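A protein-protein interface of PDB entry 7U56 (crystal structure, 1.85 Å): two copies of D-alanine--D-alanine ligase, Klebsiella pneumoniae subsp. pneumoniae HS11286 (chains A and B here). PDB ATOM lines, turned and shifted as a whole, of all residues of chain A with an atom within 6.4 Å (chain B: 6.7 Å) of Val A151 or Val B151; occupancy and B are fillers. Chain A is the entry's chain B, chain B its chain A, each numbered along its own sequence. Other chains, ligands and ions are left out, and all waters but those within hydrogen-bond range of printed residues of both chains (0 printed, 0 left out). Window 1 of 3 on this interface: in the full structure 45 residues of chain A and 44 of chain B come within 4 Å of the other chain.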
ATOM      1  N   ASP A 132      25.364 -29.332 -19.991  1.00  0.00           N
ATOM      2  CA  ASP A 132      24.575 -30.478 -19.562  1.00  0.00           C
ATOM      3  C   ASP A 132      23.319 -30.073 -18.800  1.00  0.00           C
ATOM      4  O   ASP A 132      22.661 -30.937 -18.214  1.00  0.00           O
ATOM      5  CB  ASP A 132      25.428 -31.442 -18.724  1.00  0.00           C
ATOM      6  CG  ASP A 132      25.785 -30.893 -17.319  1.00  0.00           C
ATOM      7  OD1 ASP A 132      25.430 -29.758 -16.946  1.00  0.00           O
ATOM      8  OD2 ASP A 132      26.469 -31.617 -16.576  1.00  0.00           O
ATOM      9  N   GLY A 133      22.965 -28.796 -18.815  1.00  0.00           N
ATOM     10  CA  GLY A 133      21.798 -28.330 -18.107  1.00  0.00           C
ATOM     11  C   GLY A 133      22.088 -27.678 -16.768  1.00  0.00           C
ATOM     12  O   GLY A 133      21.215 -27.000 -16.237  1.00  0.00           O
ATOM     13  N   SER A 134      23.286 -27.861 -16.213  1.00  0.00           N
ATOM     14  CA  SER A 134      23.579 -27.262 -14.914  1.00  0.00           C
ATOM     15  C   SER A 134      23.616 -25.742 -15.014  1.00  0.00           C
ATOM     16  O   SER A 134      22.983 -25.038 -14.215  1.00  0.00           O
ATOM     17  CB  SER A 134      24.910 -27.804 -14.373  1.00  0.00           C
ATOM     18  OG  SER A 134      24.832 -29.211 -14.168  1.00  0.00           O
ATOM     19  N   GLN A 136      22.286 -23.917 -17.349  1.00  0.00           N
ATOM     20  CA  GLN A 136      20.921 -23.509 -17.658  1.00  0.00           C
ATOM     21  C   GLN A 136      20.054 -23.499 -16.407  1.00  0.00           C
ATOM     22  O   GLN A 136      19.203 -22.614 -16.243  1.00  0.00           O
ATOM     23  CB  GLN A 136      20.319 -24.439 -18.716  1.00  0.00           C
ATOM     24  CG  GLN A 136      20.999 -24.357 -20.118  1.00  0.00           C
ATOM     25  CD  GLN A 136      22.397 -24.959 -20.171  1.00  0.00           C
ATOM     26  OE1 GLN A 136      22.766 -25.788 -19.341  1.00  0.00           O
ATOM     27  NE2 GLN A 136      23.178 -24.551 -21.169  1.00  0.00           N
ATOM     28  N   GLY A 137      20.250 -24.477 -15.517  1.00  0.00           N
ATOM     29  CA  GLY A 137      19.511 -24.478 -14.256  1.00  0.00           C
ATOM     30  C   GLY A 137      19.817 -23.255 -13.402  1.00  0.00           C
ATOM     31  O   GLY A 137      18.907 -22.623 -12.851  1.00  0.00           O
ATOM     32  N   MET A 138      21.100 -22.899 -13.285  1.00  0.00           N
ATOM     33  CA  MET A 138      21.465 -21.687 -12.557  1.00  0.00           C
ATOM     34  C   MET A 138      20.825 -20.437 -13.165  1.00  0.00           C
ATOM     35  O   MET A 138      20.334 -19.563 -12.438  1.00  0.00           O
ATOM     36  CB  MET A 138      22.983 -21.549 -12.532  1.00  0.00           C
ATOM     37  CG  MET A 138      23.445 -20.200 -12.028  1.00  0.00           C
ATOM     38  SD  MET A 138      25.231 -20.125 -12.120  1.00  0.00           S
ATOM     39  CE  MET A 138      25.494 -18.342 -11.968  1.00  0.00           C
ATOM     40  N   ARG A 140      18.042 -20.257 -14.993  1.00  0.00           N
ATOM     41  CA  ARG A 140      16.633 -20.335 -14.634  1.00  0.00           C
ATOM     42  C   ARG A 140      16.384 -19.886 -13.199  1.00  0.00           C
ATOM     43  O   ARG A 140      15.407 -19.175 -12.927  1.00  0.00           O
ATOM     44  CB  ARG A 140      16.135 -21.766 -14.813  1.00  0.00           C
ATOM     45  CG  ARG A 140      15.650 -22.058 -16.181  1.00  0.00           C
ATOM     46  CD  ARG A 140      15.057 -23.434 -16.188  1.00  0.00           C
ATOM     47  NE  ARG A 140      13.986 -23.614 -15.219  1.00  0.00           N
ATOM     48  CZ  ARG A 140      12.697 -23.563 -15.515  1.00  0.00           C
ATOM     49  NH1 ARG A 140      12.284 -23.234 -16.727  1.00  0.00           N
ATOM     50  NH2 ARG A 140      11.802 -23.858 -14.576  1.00  0.00           N
ATOM     51  N   PHE A 146      17.832 -16.888 -21.704  1.00  0.00           N
ATOM     52  CA  PHE A 146      19.134 -17.313 -22.224  1.00  0.00           C
ATOM     53  C   PHE A 146      18.969 -18.041 -23.551  1.00  0.00           C
ATOM     54  O   PHE A 146      17.928 -18.646 -23.826  1.00  0.00           O
ATOM     55  CB  PHE A 146      19.918 -18.187 -21.225  1.00  0.00           C
ATOM     56  CG  PHE A 146      19.192 -19.453 -20.793  1.00  0.00           C
ATOM     57  CD1 PHE A 146      19.305 -20.623 -21.527  1.00  0.00           C
ATOM     58  CD2 PHE A 146      18.433 -19.473 -19.626  1.00  0.00           C
ATOM     59  CE1 PHE A 146      18.639 -21.780 -21.120  1.00  0.00           C
ATOM     60  CE2 PHE A 146      17.769 -20.624 -19.223  1.00  0.00           C
ATOM     61  CZ  PHE A 146      17.884 -21.774 -19.966  1.00  0.00           C
ATOM     62  N   SER A 149      19.101 -24.270 -25.630  1.00  0.00           N
ATOM     63  CA  SER A 149      18.144 -25.203 -25.075  1.00  0.00           C
ATOM     64  C   SER A 149      17.996 -25.042 -23.558  1.00  0.00           C
ATOM     65  O   SER A 149      18.917 -24.630 -22.847  1.00  0.00           O
ATOM     66  CB  SER A 149      18.550 -26.634 -25.417  1.00  0.00           C
ATOM     67  OG  SER A 149      18.481 -26.876 -26.824  1.00  0.00           O
ATOM     68  N   ASP A 150      16.831 -25.419 -23.067  1.00  0.00           N
ATOM     69  CA  ASP A 150      16.534 -25.284 -21.642  1.00  0.00           C
ATOM     70  C   ASP A 150      17.179 -26.453 -20.888  1.00  0.00           C
ATOM     71  O   ASP A 150      17.990 -27.202 -21.443  1.00  0.00           O
ATOM     72  CB  ASP A 150      15.025 -25.194 -21.431  1.00  0.00           C
ATOM     73  CG  ASP A 150      14.632 -24.367 -20.207  1.00  0.00           C
ATOM     74  OD1 ASP A 150      15.471 -24.083 -19.332  1.00  0.00           O
ATOM     75  OD2 ASP A 150      13.442 -24.006 -20.127  1.00  0.00           O
ATOM     76  N   VAL A 151      16.854 -26.604 -19.591  1.00  0.00           N
ATOM     77  CA  VAL A 151      17.528 -27.598 -18.753  1.00  0.00           C
ATOM     78  C   VAL A 151      17.364 -28.995 -19.341  1.00  0.00           C
ATOM     79  O   VAL A 151      18.340 -29.738 -19.502  1.00  0.00           O
ATOM     80  CB  VAL A 151      16.982 -27.553 -17.308  1.00  0.00           C
ATOM     81  CG1 VAL A 151      17.579 -28.669 -16.490  1.00  0.00           C
ATOM     82  CG2 VAL A 151      17.271 -26.201 -16.646  1.00  0.00           C
ATOM     83  N   LEU A 152      16.114 -29.393 -19.615  1.00  0.00           N
ATOM     84  CA  LEU A 152      15.887 -30.771 -20.053  1.00  0.00           C
ATOM     85  C   LEU A 152      16.476 -31.017 -21.437  1.00  0.00           C
ATOM     86  O   LEU A 152      17.123 -32.048 -21.683  1.00  0.00           O
ATOM     87  CB  LEU A 152      14.393 -31.082 -20.041  1.00  0.00           C
ATOM     88  CG  LEU A 152      13.997 -32.470 -20.557  1.00  0.00           C
ATOM     89  CD1 LEU A 152      14.795 -33.568 -19.837  1.00  0.00           C
ATOM     90  CD2 LEU A 152      12.478 -32.661 -20.381  1.00  0.00           C
ATOM     91  N   GLY A 153      16.240 -30.100 -22.378  1.00  0.00           N
ATOM     92  CA  GLY A 153      16.803 -30.306 -23.704  1.00  0.00           C
ATOM     93  C   GLY A 153      18.318 -30.404 -23.680  1.00  0.00           C
ATOM     94  O   GLY A 153      18.911 -31.248 -24.365  1.00  0.00           O
ATOM     95  N   SER A 154      18.967 -29.516 -22.916  1.00  0.00           N
ATOM     96  CA  SER A 154      20.426 -29.558 -22.770  1.00  0.00           C
ATOM     97  C   SER A 154      20.891 -30.882 -22.160  1.00  0.00           C
ATOM     98  O   SER A 154      21.807 -31.541 -22.682  1.00  0.00           O
ATOM     99  CB  SER A 154      20.893 -28.384 -21.892  1.00  0.00           C
ATOM    100  OG  SER A 154      20.609 -27.151 -22.520  1.00  0.00           O
ATOM    101  N   ALA A 155      20.292 -31.271 -21.026  1.00  0.00           N
ATOM    102  CA  ALA A 155      20.706 -32.487 -20.344  1.00  0.00           C
ATOM    103  C   ALA A 155      20.444 -33.723 -21.194  1.00  0.00           C
ATOM    104  O   ALA A 155      21.261 -34.650 -21.212  1.00  0.00           O
ATOM    105  CB  ALA A 155      19.986 -32.587 -18.997  1.00  0.00           C
ATOM    106  N   ALA A 156      19.298 -33.771 -21.877  1.00  0.00           N
ATOM    107  CA  ALA A 156      18.959 -34.945 -22.679  1.00  0.00           C
ATOM    108  C   ALA A 156      19.870 -35.073 -23.902  1.00  0.00           C
ATOM    109  O   ALA A 156      20.359 -36.162 -24.200  1.00  0.00           O
ATOM    110  CB  ALA A 156      17.488 -34.891 -23.097  1.00  0.00           C
ATOM    111  N   ARG A 372      11.071 -17.146 -26.008  1.00  0.00           N
ATOM    112  CA  ARG A 372      10.810 -18.275 -25.125  1.00  0.00           C
ATOM    113  C   ARG A 372      10.564 -17.815 -23.688  1.00  0.00           C
ATOM    114  O   ARG A 372       9.660 -18.319 -23.014  1.00  0.00           O
ATOM    115  CB  ARG A 372      11.970 -19.272 -25.180  1.00  0.00           C
ATOM    116  CG  ARG A 372      11.686 -20.548 -24.363  1.00  0.00           C
ATOM    117  CD  ARG A 372      12.760 -21.595 -24.566  1.00  0.00           C
ATOM    118  NE  ARG A 372      14.028 -21.184 -23.969  1.00  0.00           N
ATOM    119  CZ  ARG A 372      14.371 -21.416 -22.711  1.00  0.00           C
ATOM    120  NH1 ARG A 372      13.522 -21.965 -21.854  1.00  0.00           N
ATOM    121  NH2 ARG A 372      15.586 -21.071 -22.295  1.00  0.00           N
ATOM    122  N   ASP B 132      12.554 -29.668 -11.001  1.00  0.00           N
ATOM    123  CA  ASP B 132      12.671 -29.824 -12.444  1.00  0.00           C
ATOM    124  C   ASP B 132      14.122 -29.756 -12.935  1.00  0.00           C
ATOM    125  O   ASP B 132      14.361 -29.570 -14.131  1.00  0.00           O
ATOM    126  CB  ASP B 132      11.809 -28.783 -13.162  1.00  0.00           C
ATOM    127  CG  ASP B 132      12.323 -27.360 -13.007  1.00  0.00           C
ATOM    128  OD1 ASP B 132      13.384 -27.136 -12.394  1.00  0.00           O
ATOM    129  OD2 ASP B 132      11.636 -26.444 -13.513  1.00  0.00           O
ATOM    130  N   GLY B 133      15.083 -29.881 -12.039  1.00  0.00           N
ATOM    131  CA  GLY B 133      16.476 -29.844 -12.390  1.00  0.00           C
ATOM    132  C   GLY B 133      17.153 -28.494 -12.222  1.00  0.00           C
ATOM    133  O   GLY B 133      18.386 -28.446 -12.184  1.00  0.00           O
ATOM    134  N   SER B 134      16.397 -27.400 -12.107  1.00  0.00           N
ATOM    135  CA  SER B 134      17.039 -26.091 -12.023  1.00  0.00           C
ATOM    136  C   SER B 134      17.812 -25.940 -10.721  1.00  0.00           C
ATOM    137  O   SER B 134      18.962 -25.493 -10.717  1.00  0.00           O
ATOM    138  CB  SER B 134      16.002 -24.974 -12.169  1.00  0.00           C
ATOM    139  OG  SER B 134      15.269 -25.119 -13.367  1.00  0.00           O
ATOM    140  N   LEU B 135      17.194 -26.318  -9.602  1.00  0.00           N
ATOM    141  CA  LEU B 135      17.875 -26.251  -8.313  1.00  0.00           C
ATOM    142  C   LEU B 135      19.096 -27.167  -8.296  1.00  0.00           C
ATOM    143  O   LEU B 135      20.177 -26.770  -7.848  1.00  0.00           O
ATOM    144  CB  LEU B 135      16.887 -26.607  -7.200  1.00  0.00           C
ATOM    145  CG  LEU B 135      17.495 -26.774  -5.808  1.00  0.00           C
ATOM    146  CD1 LEU B 135      18.158 -25.487  -5.351  1.00  0.00           C
ATOM    147  CD2 LEU B 135      16.387 -27.189  -4.829  1.00  0.00           C
ATOM    148  N   GLN B 136      18.943 -28.385  -8.818  1.00  0.00           N
ATOM    149  CA  GLN B 136      20.065 -29.310  -8.932  1.00  0.00           C
ATOM    150  C   GLN B 136      21.181 -28.709  -9.774  1.00  0.00           C
ATOM    151  O   GLN B 136      22.370 -28.848  -9.443  1.00  0.00           O
ATOM    152  CB  GLN B 136      19.586 -30.626  -9.551  1.00  0.00           C
ATOM    153  CG  GLN B 136      18.624 -31.445  -8.642  1.00  0.00           C
ATOM    154  CD  GLN B 136      17.207 -30.878  -8.533  1.00  0.00           C
ATOM    155  OE1 GLN B 136      16.772 -30.066  -9.350  1.00  0.00           O
ATOM    156  NE2 GLN B 136      16.476 -31.323  -7.516  1.00  0.00           N
ATOM    157  N   GLY B 137      20.820 -28.034 -10.861  1.00  0.00           N
ATOM    158  CA  GLY B 137      21.843 -27.404 -11.681  1.00  0.00           C
ATOM    159  C   GLY B 137      22.606 -26.322 -10.942  1.00  0.00           C
ATOM    160  O   GLY B 137      23.828 -26.209 -11.067  1.00  0.00           O
ATOM    161  N   MET B 138      21.900 -25.508 -10.161  1.00  0.00           N
ATOM    162  CA  MET B 138      22.589 -24.486  -9.382  1.00  0.00           C
ATOM    163  C   MET B 138      23.516 -25.107  -8.335  1.00  0.00           C
ATOM    164  O   MET B 138      24.641 -24.631  -8.120  1.00  0.00           O
ATOM    165  CB  MET B 138      21.574 -23.556  -8.723  1.00  0.00           C
ATOM    166  CG  MET B 138      22.265 -22.342  -8.164  1.00  0.00           C
ATOM    167  SD  MET B 138      21.159 -21.379  -7.132  1.00  0.00           S
ATOM    168  CE  MET B 138      21.177 -22.416  -5.668  1.00  0.00           C
ATOM    169  N   ARG B 140      24.977 -27.957  -8.565  1.00  0.00           N
ATOM    170  CA  ARG B 140      26.138 -28.460  -9.293  1.00  0.00           C
ATOM    171  C   ARG B 140      27.118 -27.343  -9.633  1.00  0.00           C
ATOM    172  O   ARG B 140      28.337 -27.551  -9.613  1.00  0.00           O
ATOM    173  CB  ARG B 140      25.689 -29.156 -10.579  1.00  0.00           C
ATOM    174  CG  ARG B 140      25.102 -30.523 -10.309  1.00  0.00           C
ATOM    175  CD  ARG B 140      24.738 -31.221 -11.573  1.00  0.00           C
ATOM    176  NE  ARG B 140      25.846 -31.333 -12.519  1.00  0.00           N
ATOM    177  CZ  ARG B 140      26.762 -32.288 -12.498  1.00  0.00           C
ATOM    178  NH1 ARG B 140      26.790 -33.199 -11.540  1.00  0.00           N
ATOM    179  NH2 ARG B 140      27.673 -32.331 -13.468  1.00  0.00           N
ATOM    180  N   PHE B 146      24.290 -33.289  -3.079  1.00  0.00           N
ATOM    181  CA  PHE B 146      22.879 -33.189  -2.721  1.00  0.00           C
ATOM    182  C   PHE B 146      22.172 -34.536  -2.846  1.00  0.00           C
ATOM    183  O   PHE B 146      22.532 -35.392  -3.661  1.00  0.00           O
ATOM    184  CB  PHE B 146      22.139 -32.116  -3.548  1.00  0.00           C
ATOM    185  CG  PHE B 146      22.198 -32.324  -5.036  1.00  0.00           C
ATOM    186  CD1 PHE B 146      21.284 -33.137  -5.679  1.00  0.00           C
ATOM    187  CD2 PHE B 146      23.158 -31.668  -5.807  1.00  0.00           C
ATOM    188  CE1 PHE B 146      21.340 -33.322  -7.081  1.00  0.00           C
ATOM    189  CE2 PHE B 146      23.216 -31.842  -7.180  1.00  0.00           C
ATOM    190  CZ  PHE B 146      22.311 -32.667  -7.826  1.00  0.00           C
ATOM    191  N   SER B 149      17.711 -37.028  -7.140  1.00  0.00           N
ATOM    192  CA  SER B 149      18.064 -37.186  -8.537  1.00  0.00           C
ATOM    193  C   SER B 149      18.835 -35.979  -9.061  1.00  0.00           C
ATOM    194  O   SER B 149      18.712 -34.862  -8.554  1.00  0.00           O
ATOM    195  CB  SER B 149      16.812 -37.421  -9.383  1.00  0.00           C
ATOM    196  OG  SER B 149      16.251 -38.695  -9.132  1.00  0.00           O
ATOM    197  N   ASP B 150      19.643 -36.214 -10.088  1.00  0.00           N
ATOM    198  CA  ASP B 150      20.500 -35.145 -10.590  1.00  0.00           C
ATOM    199  C   ASP B 150      19.720 -34.334 -11.632  1.00  0.00           C
ATOM    200  O   ASP B 150      18.499 -34.444 -11.729  1.00  0.00           O
ATOM    201  CB  ASP B 150      21.819 -35.723 -11.125  1.00  0.00           C
ATOM    202  CG  ASP B 150      22.968 -34.709 -11.051  1.00  0.00           C
ATOM    203  OD1 ASP B 150      22.885 -33.658 -11.725  1.00  0.00           O
ATOM    204  OD2 ASP B 150      23.933 -34.930 -10.277  1.00  0.00           O
ATOM    205  N   VAL B 151      20.422 -33.510 -12.426  1.00  0.00           N
ATOM    206  CA  VAL B 151      19.750 -32.583 -13.336  1.00  0.00           C
ATOM    207  C   VAL B 151      18.871 -33.327 -14.332  1.00  0.00           C
ATOM    208  O   VAL B 151      17.685 -33.015 -14.493  1.00  0.00           O
ATOM    209  CB  VAL B 151      20.786 -31.700 -14.064  1.00  0.00           C
ATOM    210  CG1 VAL B 151      20.091 -30.874 -15.150  1.00  0.00           C
ATOM    211  CG2 VAL B 151      21.508 -30.803 -13.085  1.00  0.00           C
ATOM    212  N   LEU B 152      19.446 -34.301 -15.039  1.00  0.00           N
ATOM    213  CA  LEU B 152      18.699 -34.984 -16.085  1.00  0.00           C
ATOM    214  C   LEU B 152      17.556 -35.800 -15.503  1.00  0.00           C
ATOM    215  O   LEU B 152      16.431 -35.738 -15.996  1.00  0.00           O
ATOM    216  CB  LEU B 152      19.627 -35.885 -16.898  1.00  0.00           C
ATOM    217  CG  LEU B 152      18.944 -36.781 -17.944  1.00  0.00           C
ATOM    218  CD1 LEU B 152      18.205 -35.966 -18.976  1.00  0.00           C
ATOM    219  CD2 LEU B 152      19.999 -37.650 -18.605  1.00  0.00           C
ATOM    220  N   GLY B 153      17.830 -36.580 -14.453  1.00  0.00           N
ATOM    221  CA  GLY B 153      16.774 -37.396 -13.875  1.00  0.00           C
ATOM    222  C   GLY B 153      15.625 -36.558 -13.343  1.00  0.00           C
ATOM    223  O   GLY B 153      14.456 -36.909 -13.517  1.00  0.00           O
ATOM    224  N   SER B 154      15.944 -35.440 -12.702  1.00  0.00           N
ATOM    225  CA  SER B 154      14.908 -34.547 -12.197  1.00  0.00           C
ATOM    226  C   SER B 154      14.093 -33.955 -13.337  1.00  0.00           C
ATOM    227  O   SER B 154      12.859 -33.982 -13.314  1.00  0.00           O
ATOM    228  CB  SER B 154      15.543 -33.442 -11.358  1.00  0.00           C
ATOM    229  OG  SER B 154      16.230 -33.981 -10.231  1.00  0.00           O
ATOM    230  N   ALA B 155      14.774 -33.371 -14.329  1.00  0.00           N
ATOM    231  CA  ALA B 155      14.092 -32.737 -15.455  1.00  0.00           C
ATOM    232  C   ALA B 155      13.237 -33.726 -16.226  1.00  0.00           C
ATOM    233  O   ALA B 155      12.101 -33.406 -16.626  1.00  0.00           O
ATOM    234  CB  ALA B 155      15.132 -32.082 -16.387  1.00  0.00           C
ATOM    235  N   ALA B 156      13.770 -34.926 -16.474  1.00  0.00           N
ATOM    236  CA  ALA B 156      13.048 -35.906 -17.280  1.00  0.00           C
ATOM    237  C   ALA B 156      11.824 -36.437 -16.544  1.00  0.00           C
ATOM    238  O   ALA B 156      10.750 -36.584 -17.144  1.00  0.00           O
ATOM    239  CB  ALA B 156      13.985 -37.053 -17.666  1.00  0.00           C
ATOM    240  N   ARG B 372      27.449 -40.716  -4.407  1.00  0.00           N
ATOM    241  CA  ARG B 372      27.325 -40.279  -5.796  1.00  0.00           C
ATOM    242  C   ARG B 372      28.229 -39.090  -6.089  1.00  0.00           C
ATOM    243  O   ARG B 372      28.809 -38.988  -7.181  1.00  0.00           O
ATOM    244  CB  ARG B 372      25.876 -39.927  -6.118  1.00  0.00           C
ATOM    245  CG  ARG B 372      25.663 -39.856  -7.629  1.00  0.00           C
ATOM    246  CD  ARG B 372      24.205 -39.712  -8.002  1.00  0.00           C
ATOM    247  NE  ARG B 372      23.655 -38.449  -7.529  1.00  0.00           N
ATOM    248  CZ  ARG B 372      23.845 -37.282  -8.116  1.00  0.00           C
ATOM    249  NH1 ARG B 372      24.569 -37.174  -9.221  1.00  0.00           N
ATOM    250  NH2 ARG B 372      23.303 -36.193  -7.578  1.00  0.00           N
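Asp A132 touches Arg B140, and with the chains exchanged Arg A140 touches Asp B132. Asp A132 touches Val B151, but with the chains exchanged Val A151 does not touch Asp B132 (4.1 Å). Val B151 touches its own counterpart, Val A151. Leu A152 touches Ala B155, and with the chains exchanged Ala A155 touches Leu B152. Of the 14 pairs that touch across the chains among the printed residues, 13 have their exchanged pair printed and touching as well.
The side-chain hydroxyl of Ser B134 is in hydrogen-bond range of the side-chain carboxylate of Asp B132 (2.9 Å). The side-chain carboxylate (OD2) of Asp B150 is in salt-bridge range of the guanidinium group (NH1) of Arg B140, 3.6 Å away. The side-chain hydroxyl (OG) of Ser A134 is in hydrogen-bond range of the side-chain carboxylate (OD1) of Asp A132 (2.9 Å). The guanidinium group (NH1) of Arg A140 is in salt-bridge range of the side-chain carboxylate (OD2) of Asp A150 (3.7 Å).
Of the 17 printed residues of chain A, 8 touch a printed residue of chain B. Hydrophobic or aromatic side chains of chain A that line the printed part of chain B: Val A151, Leu A152 and Ala A155. Hydrophobic or aromatic side chains of chain B within 4 Å of the printed part of chain A: Val B151, Leu B152 and Ala B155.
Printed residues of chain B within 4 Å of Val A151: Ser B134 and Val B151. Printed residues of chain A within 4 Å of Val B151: Asp A132, Ser A134 and Val A151. Printed residues of chain A within 4 Å of Ala B155: Leu A152. Printed residues of chain B within 4 Å of Ser A134: Gly B137, Arg B140 and Val B151. Printed residues of chain A within 4 Å of Arg B140: Asp A132 and Ser A134. Printed residues of chain A within 4 Å of Leu B152: Ala A155 (3.8 Å) and Ala A156 (3.8 Å). Of the printed residues of chain B, Arg A140 touches Asp B132 and Ser B134. Gln A136 touches none of the printed residues of chain B. The nearest printed residue of chain B that does not touch Val A151 is Asp B132 (4.1 Å). The nearest printed residue of chain A that does not touch Val B151 is Gly A133 (4.1 Å).
The guanidinium group (NH2) of Arg A140 lies within salt-bridge range of the side-chain carboxylate (OD2) of Asp B132 (2.8 Å). OG of Ser B134 sits at hydrogen-bond distance from NE of Arg A140. The guanidinium group of Arg B140 lies within salt-bridge range of the side-chain carboxylate of Asp A132. NE of Arg B140 lies within hydrogen-bond range of OG of Ser A134 (2.9 Å). The backbone carbonyl oxygen (O) of Ser A134 sits close to the backbone carbonyl oxygen (O) of Gly B137, at 3.5 Å.
Val B151 touches Asp A132. Ser A134 touches Val B151. Gly A137 touches Ser B134. CG2 of Val A151 touches OG of Ser B134, at 3.99 Å. Val A151 touches Val B151. CB of Ala B155 touches CD1 of Leu A152, 3.8 Å away. Ala B156 touches Leu A152 (N to CD1, 3.8 Å). Leu B152 touches Ala A155 (CD1 to CB, 3.8 Å). Leu B152 touches Ala A156.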
